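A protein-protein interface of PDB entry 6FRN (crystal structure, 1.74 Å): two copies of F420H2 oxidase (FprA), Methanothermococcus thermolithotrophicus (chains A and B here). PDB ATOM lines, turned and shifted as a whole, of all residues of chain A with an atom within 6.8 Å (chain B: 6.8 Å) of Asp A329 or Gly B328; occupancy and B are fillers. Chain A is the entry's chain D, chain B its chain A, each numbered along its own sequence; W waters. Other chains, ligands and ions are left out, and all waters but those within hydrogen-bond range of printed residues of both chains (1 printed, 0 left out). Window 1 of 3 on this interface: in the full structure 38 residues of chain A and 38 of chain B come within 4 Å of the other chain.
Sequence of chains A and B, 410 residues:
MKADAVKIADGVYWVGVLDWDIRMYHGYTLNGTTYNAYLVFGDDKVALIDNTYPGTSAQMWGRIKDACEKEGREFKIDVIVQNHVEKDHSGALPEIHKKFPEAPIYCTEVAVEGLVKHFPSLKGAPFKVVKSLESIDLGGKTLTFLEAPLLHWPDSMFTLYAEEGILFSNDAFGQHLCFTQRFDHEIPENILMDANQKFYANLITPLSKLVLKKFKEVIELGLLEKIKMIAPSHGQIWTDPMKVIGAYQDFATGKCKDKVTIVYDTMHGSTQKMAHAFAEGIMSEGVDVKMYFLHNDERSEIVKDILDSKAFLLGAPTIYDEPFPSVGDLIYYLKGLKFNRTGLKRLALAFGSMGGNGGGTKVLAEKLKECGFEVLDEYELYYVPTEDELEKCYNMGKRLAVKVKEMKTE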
ATOM      1  N   LEU A 294      22.334   5.505   6.348  1.00  0.00           N
ATOM      2  CA  LEU A 294      22.483   4.052   6.234  1.00  0.00           C
ATOM      3  C   LEU A 294      21.533   3.221   7.063  1.00  0.00           C
ATOM      4  O   LEU A 294      21.346   2.046   6.741  1.00  0.00           O
ATOM      5  CB  LEU A 294      23.906   3.597   6.535  1.00  0.00           C
ATOM      6  CG  LEU A 294      24.925   3.943   5.503  1.00  0.00           C
ATOM      7  CD1 LEU A 294      26.336   3.716   6.042  1.00  0.00           C
ATOM      8  CD2 LEU A 294      24.717   3.145   4.200  1.00  0.00           C
ATOM      9  N   ARG A 299      22.044   0.588  -0.564  1.00  0.00           N
ATOM     10  CA  ARG A 299      23.345   0.677  -1.239  1.00  0.00           C
ATOM     11  C   ARG A 299      23.190   0.967  -2.739  1.00  0.00           C
ATOM     12  O   ARG A 299      24.014   1.664  -3.317  1.00  0.00           O
ATOM     13  CB  ARG A 299      24.188  -0.588  -1.013  1.00  0.00           C
ATOM     14  CG  ARG A 299      23.714  -1.833  -1.759  1.00  0.00           C
ATOM     15  CD  ARG A 299      24.559  -3.030  -1.445  1.00  0.00           C
ATOM     16  NE  ARG A 299      24.260  -3.673  -0.157  1.00  0.00           N
ATOM     17  CZ  ARG A 299      23.279  -4.544   0.064  1.00  0.00           C
ATOM     18  NH1 ARG A 299      23.133  -5.101   1.263  1.00  0.00           N
ATOM     19  NH2 ARG A 299      22.429  -4.860  -0.906  1.00  0.00           N
ATOM     20  N   PRO A 325      28.890  -0.480  12.213  1.00  0.00           N
ATOM     21  CA  PRO A 325      29.082  -1.548  11.216  1.00  0.00           C
ATOM     22  C   PRO A 325      28.356  -1.457   9.894  1.00  0.00           C
ATOM     23  O   PRO A 325      28.828  -2.086   8.948  1.00  0.00           O
ATOM     24  CB  PRO A 325      28.707  -2.810  11.976  1.00  0.00           C
ATOM     25  CG  PRO A 325      27.809  -2.334  13.048  1.00  0.00           C
ATOM     26  CD  PRO A 325      28.452  -1.066  13.494  1.00  0.00           C
ATOM     27  N   SER A 326      27.246  -0.709   9.791  1.00  0.00           N
ATOM     28  CA  SER A 326      26.527  -0.546   8.536  1.00  0.00           C
ATOM     29  C   SER A 326      27.414  -0.027   7.406  1.00  0.00           C
ATOM     30  O   SER A 326      27.168  -0.345   6.231  1.00  0.00           O
ATOM     31  CB  SER A 326      25.356   0.405   8.730  1.00  0.00           C
ATOM     32  OG  SER A 326      25.897   1.633   9.197  1.00  0.00           O
ATOM     33  N   VAL A 327      28.489   0.729   7.743  1.00  0.00           N
ATOM     34  CA  VAL A 327      29.412   1.219   6.716  1.00  0.00           C
ATOM     35  C   VAL A 327      30.164   0.079   6.033  1.00  0.00           C
ATOM     36  O   VAL A 327      30.606   0.247   4.911  1.00  0.00           O
ATOM     37  CB  VAL A 327      30.425   2.281   7.238  1.00  0.00           C
ATOM     38  CG1 VAL A 327      29.718   3.447   7.913  1.00  0.00           C
ATOM     39  CG2 VAL A 327      31.475   1.669   8.146  1.00  0.00           C
ATOM     40  N   GLY A 328      30.369  -1.038   6.736  1.00  0.00           N
ATOM     41  CA  GLY A 328      31.080  -2.181   6.182  1.00  0.00           C
ATOM     42  C   GLY A 328      30.389  -2.774   4.979  1.00  0.00           C
ATOM     43  O   GLY A 328      31.043  -3.301   4.076  1.00  0.00           O
ATOM     44  N   ASP A 329      29.038  -2.709   4.940  1.00  0.00           N
ATOM     45  CA  ASP A 329      28.300  -3.228   3.816  1.00  0.00           C
ATOM     46  C   ASP A 329      28.568  -2.354   2.606  1.00  0.00           C
ATOM     47  O   ASP A 329      28.955  -2.850   1.539  1.00  0.00           O
ATOM     48  CB  ASP A 329      26.805  -3.281   4.163  1.00  0.00           C
ATOM     49  CG  ASP A 329      25.886  -3.654   3.032  1.00  0.00           C
ATOM     50  OD1 ASP A 329      25.950  -2.995   1.957  1.00  0.00           O
ATOM     51  OD2 ASP A 329      25.048  -4.529   3.231  1.00  0.00           O
ATOM     52  N   LEU A 330      28.473  -1.054   2.786  1.00  0.00           N
ATOM     53  CA  LEU A 330      28.706  -0.147   1.664  1.00  0.00           C
ATOM     54  C   LEU A 330      30.150  -0.217   1.204  1.00  0.00           C
ATOM     55  O   LEU A 330      30.391  -0.249   0.000  1.00  0.00           O
ATOM     56  CB  LEU A 330      28.337   1.296   2.046  1.00  0.00           C
ATOM     57  CG  LEU A 330      28.542   2.339   0.942  1.00  0.00           C
ATOM     58  CD1 LEU A 330      27.747   2.024  -0.290  1.00  0.00           C
ATOM     59  CD2 LEU A 330      28.234   3.692   1.458  1.00  0.00           C
ATOM     60  N   ILE A 331      31.102  -0.273   2.145  1.00  0.00           N
ATOM     61  CA  ILE A 331      32.527  -0.384   1.822  1.00  0.00           C
ATOM     62  C   ILE A 331      32.806  -1.679   1.006  1.00  0.00           C
ATOM     63  O   ILE A 331      33.496  -1.626  -0.010  1.00  0.00           O
ATOM     64  CB  ILE A 331      33.410  -0.272   3.080  1.00  0.00           C
ATOM     65  CG1 ILE A 331      33.423   1.180   3.577  1.00  0.00           C
ATOM     66  CG2 ILE A 331      34.850  -0.771   2.801  1.00  0.00           C
ATOM     67  CD1 ILE A 331      33.905   1.325   5.001  1.00  0.00           C
ATOM     68  N   TYR A 332      32.262  -2.802   1.419  1.00  0.00           N
ATOM     69  CA  TYR A 332      32.437  -4.061   0.649  1.00  0.00           C
ATOM     70  C   TYR A 332      31.876  -3.932  -0.773  1.00  0.00           C
ATOM     71  O   TYR A 332      32.458  -4.433  -1.718  1.00  0.00           O
ATOM     72  CB  TYR A 332      31.784  -5.242   1.363  1.00  0.00           C
ATOM     73  CG  TYR A 332      32.688  -5.916   2.373  1.00  0.00           C
ATOM     74  CD1 TYR A 332      33.474  -5.171   3.246  1.00  0.00           C
ATOM     75  CD2 TYR A 332      32.689  -7.300   2.521  1.00  0.00           C
ATOM     76  CE1 TYR A 332      34.265  -5.790   4.207  1.00  0.00           C
ATOM     77  CE2 TYR A 332      33.525  -7.929   3.439  1.00  0.00           C
ATOM     78  CZ  TYR A 332      34.358  -7.174   4.238  1.00  0.00           C
ATOM     79  OH  TYR A 332      35.097  -7.805   5.201  1.00  0.00           O
ATOM     80  N   TYR A 333      30.741  -3.267  -0.918  1.00  0.00           N
ATOM     81  CA  TYR A 333      30.119  -3.060  -2.213  1.00  0.00           C
ATOM     82  C   TYR A 333      30.955  -2.138  -3.068  1.00  0.00           C
ATOM     83  O   TYR A 333      31.221  -2.468  -4.234  1.00  0.00           O
ATOM     84  CB  TYR A 333      28.716  -2.489  -2.022  1.00  0.00           C
ATOM     85  CG  TYR A 333      27.807  -2.598  -3.217  1.00  0.00           C
ATOM     86  CD1 TYR A 333      27.579  -3.830  -3.833  1.00  0.00           C
ATOM     87  CD2 TYR A 333      26.996  -1.533  -3.594  1.00  0.00           C
ATOM     88  CE1 TYR A 333      26.640  -3.969  -4.844  1.00  0.00           C
ATOM     89  CE2 TYR A 333      26.041  -1.671  -4.593  1.00  0.00           C
ATOM     90  CZ  TYR A 333      25.872  -2.894  -5.222  1.00  0.00           C
ATOM     91  OH  TYR A 333      24.910  -3.078  -6.192  1.00  0.00           O
ATOM     92  N   LEU A 334      31.470  -1.037  -2.485  1.00  0.00           N
ATOM     93  CA  LEU A 334      32.359  -0.127  -3.225  1.00  0.00           C
ATOM     94  C   LEU A 334      33.687  -0.800  -3.628  1.00  0.00           C
ATOM     95  O   LEU A 334      34.234  -0.482  -4.681  1.00  0.00           O
ATOM     96  CB  LEU A 334      32.671   1.133  -2.396  1.00  0.00           C
ATOM     97  CG  LEU A 334      31.498   2.070  -2.184  1.00  0.00           C
ATOM     98  CD1 LEU A 334      31.860   3.139  -1.195  1.00  0.00           C
ATOM     99  CD2 LEU A 334      31.051   2.728  -3.524  1.00  0.00           C
ATOM    100  N   LEU B 294      21.302 -13.378   6.167  1.00  0.00           N
ATOM    101  CA  LEU B 294      21.601 -11.944   6.277  1.00  0.00           C
ATOM    102  C   LEU B 294      20.661 -11.024   5.542  1.00  0.00           C
ATOM    103  O   LEU B 294      20.609  -9.842   5.873  1.00  0.00           O
ATOM    104  CB  LEU B 294      23.040 -11.624   5.864  1.00  0.00           C
ATOM    105  CG  LEU B 294      24.117 -12.078   6.798  1.00  0.00           C
ATOM    106  CD1 LEU B 294      25.481 -11.986   6.140  1.00  0.00           C
ATOM    107  CD2 LEU B 294      24.112 -11.277   8.104  1.00  0.00           C
ATOM    108  N   PRO B 323      32.885 -10.832  -1.546  1.00  0.00           N
ATOM    109  CA  PRO B 323      31.708 -11.521  -1.031  1.00  0.00           C
ATOM    110  C   PRO B 323      30.520 -10.565  -1.025  1.00  0.00           C
ATOM    111  O   PRO B 323      30.728  -9.351  -0.953  1.00  0.00           O
ATOM    112  CB  PRO B 323      32.113 -11.923   0.378  1.00  0.00           C
ATOM    113  CG  PRO B 323      33.177 -10.979   0.769  1.00  0.00           C
ATOM    114  CD  PRO B 323      33.851 -10.500  -0.466  1.00  0.00           C
ATOM    115  N   PHE B 324      29.284 -11.109  -1.099  1.00  0.00           N
ATOM    116  CA  PHE B 324      28.043 -10.319  -1.061  1.00  0.00           C
ATOM    117  C   PHE B 324      28.127  -9.283   0.066  1.00  0.00           C
ATOM    118  O   PHE B 324      28.511  -9.653   1.176  1.00  0.00           O
ATOM    119  CB  PHE B 324      26.812 -11.213  -0.986  1.00  0.00           C
ATOM    120  CG  PHE B 324      25.565 -10.434  -1.285  1.00  0.00           C
ATOM    121  CD1 PHE B 324      25.212 -10.135  -2.596  1.00  0.00           C
ATOM    122  CD2 PHE B 324      24.858  -9.821  -0.268  1.00  0.00           C
ATOM    123  CE1 PHE B 324      24.136  -9.302  -2.869  1.00  0.00           C
ATOM    124  CE2 PHE B 324      23.756  -9.022  -0.542  1.00  0.00           C
ATOM    125  CZ  PHE B 324      23.424  -8.737  -1.836  1.00  0.00           C
ATOM    126  N   PRO B 325      27.846  -7.978  -0.184  1.00  0.00           N
ATOM    127  CA  PRO B 325      28.255  -6.954   0.792  1.00  0.00           C
ATOM    128  C   PRO B 325      27.645  -6.980   2.165  1.00  0.00           C
ATOM    129  O   PRO B 325      28.225  -6.388   3.065  1.00  0.00           O
ATOM    130  CB  PRO B 325      27.955  -5.639   0.079  1.00  0.00           C
ATOM    131  CG  PRO B 325      26.900  -6.001  -0.917  1.00  0.00           C
ATOM    132  CD  PRO B 325      27.362  -7.328  -1.421  1.00  0.00           C
ATOM    133  N   SER B 326      26.500  -7.631   2.360  1.00  0.00           N
ATOM    134  CA  SER B 326      25.880  -7.723   3.683  1.00  0.00           C
ATOM    135  C   SER B 326      26.816  -8.337   4.714  1.00  0.00           C
ATOM    136  O   SER B 326      26.727  -7.984   5.891  1.00  0.00           O
ATOM    137  CB  SER B 326      24.599  -8.551   3.589  1.00  0.00           C
ATOM    138  OG  SER B 326      24.980  -9.824   3.090  1.00  0.00           O
ATOM    139  N   VAL B 327      27.779  -9.201   4.278  1.00  0.00           N
ATOM    140  CA  VAL B 327      28.741  -9.798   5.205  1.00  0.00           C
ATOM    141  C   VAL B 327      29.693  -8.740   5.806  1.00  0.00           C
ATOM    142  O   VAL B 327      30.227  -8.955   6.879  1.00  0.00           O
ATOM    143  CB  VAL B 327      29.583 -10.953   4.601  1.00  0.00           C
ATOM    144  CG1 VAL B 327      28.700 -12.032   3.991  1.00  0.00           C
ATOM    145  CG2 VAL B 327      30.605 -10.443   3.608  1.00  0.00           C
ATOM    146  N   GLY B 328      29.932  -7.656   5.094  1.00  0.00           N
ATOM    147  CA  GLY B 328      30.807  -6.594   5.557  1.00  0.00           C
ATOM    148  C   GLY B 328      30.298  -5.931   6.819  1.00  0.00           C
ATOM    149  O   GLY B 328      31.095  -5.479   7.641  1.00  0.00           O
ATOM    150  N   ASP B 329      28.981  -5.864   6.989  1.00  0.00           N
ATOM    151  CA  ASP B 329      28.405  -5.274   8.170  1.00  0.00           C
ATOM    152  C   ASP B 329      28.682  -6.181   9.346  1.00  0.00           C
ATOM    153  O   ASP B 329      29.205  -5.731  10.369  1.00  0.00           O
ATOM    154  CB  ASP B 329      26.885  -5.060   7.955  1.00  0.00           C
ATOM    155  CG  ASP B 329      26.127  -4.595   9.153  1.00  0.00           C
ATOM    156  OD1 ASP B 329      26.217  -5.256  10.216  1.00  0.00           O
ATOM    157  OD2 ASP B 329      25.448  -3.588   9.047  1.00  0.00           O
ATOM    158  N   LEU B 330      28.417  -7.461   9.180  1.00  0.00           N
ATOM    159  CA  LEU B 330      28.664  -8.415  10.267  1.00  0.00           C
ATOM    160  C   LEU B 330      30.158  -8.488  10.596  1.00  0.00           C
ATOM    161  O   LEU B 330      30.510  -8.488  11.769  1.00  0.00           O
ATOM    162  CB  LEU B 330      28.104  -9.797   9.921  1.00  0.00           C
ATOM    163  CG  LEU B 330      28.306 -10.862  11.003  1.00  0.00           C
ATOM    164  CD1 LEU B 330      27.661 -10.476  12.296  1.00  0.00           C
ATOM    165  CD2 LEU B 330      27.797 -12.194  10.512  1.00  0.00           C
ATOM    166  N   ILE B 331      31.021  -8.500   9.588  1.00  0.00           N
ATOM    167  CA  ILE B 331      32.470  -8.539   9.785  1.00  0.00           C
ATOM    168  C   ILE B 331      32.957  -7.286  10.566  1.00  0.00           C
ATOM    169  O   ILE B 331      33.729  -7.415  11.511  1.00  0.00           O
ATOM    170  CB  ILE B 331      33.220  -8.733   8.457  1.00  0.00           C
ATOM    171  CG1 ILE B 331      33.037 -10.187   7.961  1.00  0.00           C
ATOM    172  CG2 ILE B 331      34.719  -8.391   8.622  1.00  0.00           C
ATOM    173  CD1 ILE B 331      33.357 -10.375   6.520  1.00  0.00           C
ATOM    174  N   TYR B 332      32.493  -6.096  10.190  1.00  0.00           N
ATOM    175  CA  TYR B 332      32.853  -4.873  10.932  1.00  0.00           C
ATOM    176  C   TYR B 332      32.408  -4.955  12.400  1.00  0.00           C
ATOM    177  O   TYR B 332      33.134  -4.517  13.291  1.00  0.00           O
ATOM    178  CB  TYR B 332      32.269  -3.633  10.293  1.00  0.00           C
ATOM    179  CG  TYR B 332      33.136  -3.048   9.197  1.00  0.00           C
ATOM    180  CD1 TYR B 332      33.750  -3.863   8.249  1.00  0.00           C
ATOM    181  CD2 TYR B 332      33.313  -1.675   9.086  1.00  0.00           C
ATOM    182  CE1 TYR B 332      34.530  -3.324   7.232  1.00  0.00           C
ATOM    183  CE2 TYR B 332      34.074  -1.127   8.063  1.00  0.00           C
ATOM    184  CZ  TYR B 332      34.716  -1.955   7.166  1.00  0.00           C
ATOM    185  OH  TYR B 332      35.394  -1.377   6.141  1.00  0.00           O
ATOM    186  N   TYR B 333      31.243  -5.519  12.649  1.00  0.00           N
ATOM    187  CA  TYR B 333      30.713  -5.668  13.988  1.00  0.00           C
ATOM    188  C   TYR B 333      31.521  -6.677  14.773  1.00  0.00           C
ATOM    189  O   TYR B 333      31.916  -6.387  15.896  1.00  0.00           O
ATOM    190  CB  TYR B 333      29.246  -6.097  13.923  1.00  0.00           C
ATOM    191  CG  TYR B 333      28.450  -5.895  15.186  1.00  0.00           C
ATOM    192  CD1 TYR B 333      28.424  -4.658  15.824  1.00  0.00           C
ATOM    193  CD2 TYR B 333      27.567  -6.872  15.635  1.00  0.00           C
ATOM    194  CE1 TYR B 333      27.582  -4.416  16.906  1.00  0.00           C
ATOM    195  CE2 TYR B 333      26.710  -6.638  16.708  1.00  0.00           C
ATOM    196  CZ  TYR B 333      26.723  -5.406  17.342  1.00  0.00           C
ATOM    197  OH  TYR B 333      25.871  -5.117  18.376  1.00  0.00           O
ATOM    198  N   LEU B 364      36.321 -13.973   2.875  1.00  0.00           N
ATOM    199  CA  LEU B 364      35.662 -14.382   4.130  1.00  0.00           C
ATOM    200  C   LEU B 364      36.641 -15.078   5.084  1.00  0.00           C
ATOM    201  O   LEU B 364      36.627 -14.805   6.274  1.00  0.00           O
ATOM    202  CB  LEU B 364      34.505 -15.339   3.835  1.00  0.00           C
ATOM    203  CG  LEU B 364      33.299 -14.776   3.081  1.00  0.00           C
ATOM    204  CD1 LEU B 364      32.302 -15.867   2.811  1.00  0.00           C
ATOM    205  CD2 LEU B 364      32.643 -13.662   3.837  1.00  0.00           C
HETATM  206  O   HOH W   1      30.536  -6.708  -2.152  1.00  0.00           O
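The backbone NH (N) of Ser A326 sits close to the side-chain carboxylate (OD2) of Asp B329, at 3.5 Å.
The guanidinium group of Arg A299 is in salt-bridge range of the side-chain carboxylate of Asp A329.
Pro B325 touches Arg A299. Tyr B332 touches Val A327. C of Gly A328 touches N of Asp B329 (3.9 Å). CA of Asp A329 touches O of Pro B325, 3.2 Å away. Asp A329 touches Gly B328 (N to C, 3.9 Å). Asp A329 touches Asp B329 (N to N, 3.8 Å). Pro B325 touches Tyr A332 (CA to CB, 3.96 Å). Val B327 touches Tyr A332 (CG2 to CE2, 3.9 Å). Tyr A332 touches Tyr B332. Tyr A333 touches Pro B325.
Asp A329 touches just these residues of chain B: Pro B325, Ser B326, Gly B328 and Asp B329. Of chain A, only Gly A328, Asp A329 and Tyr A332 come within 4 Å of Gly B328. Of the printed residues of chain A, Tyr B333 touches Pro A325. Of the printed residues of chain A, Ile B331 touches Tyr A332. Leu B294 touches none of the printed residues of chain A. Leu B330 touches none of the printed residues of chain A. The nearest residue of chain B that does not touch Asp A329 is Val B327 (5.5 Å).
Hydrophobic or aromatic side chains of chain A within 4 Å of the printed part of chain B: Pro A325, Val A327, Ile A331, Tyr A332 and Tyr A333. Along chain A the printed residues that touch a printed residue of chain B span positions 299 to 333. Hydrophobic or aromatic side chains of chain B that line the printed part of chain A: Pro B325, Val B327, Ile B331, Tyr B332 and Tyr B333.
Pro A325 touches Asp B329, and with the chains exchanged Asp A329 touches Pro B325. Pro A325 touches Tyr B332, and with the chains exchanged Tyr A332 touches Pro B325. Gly A328 touches Tyr B332, and with the chains exchanged Tyr A332 touches Gly B328. Tyr A332 touches its own counterpart, Tyr B332. 10 positions are printed for both chains.
Water W1 bridges the backbone carbonyl oxygen of Pro B323 (2.9 Å) and the backbone carbonyl oxygen of Tyr A332 (3.0 Å).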
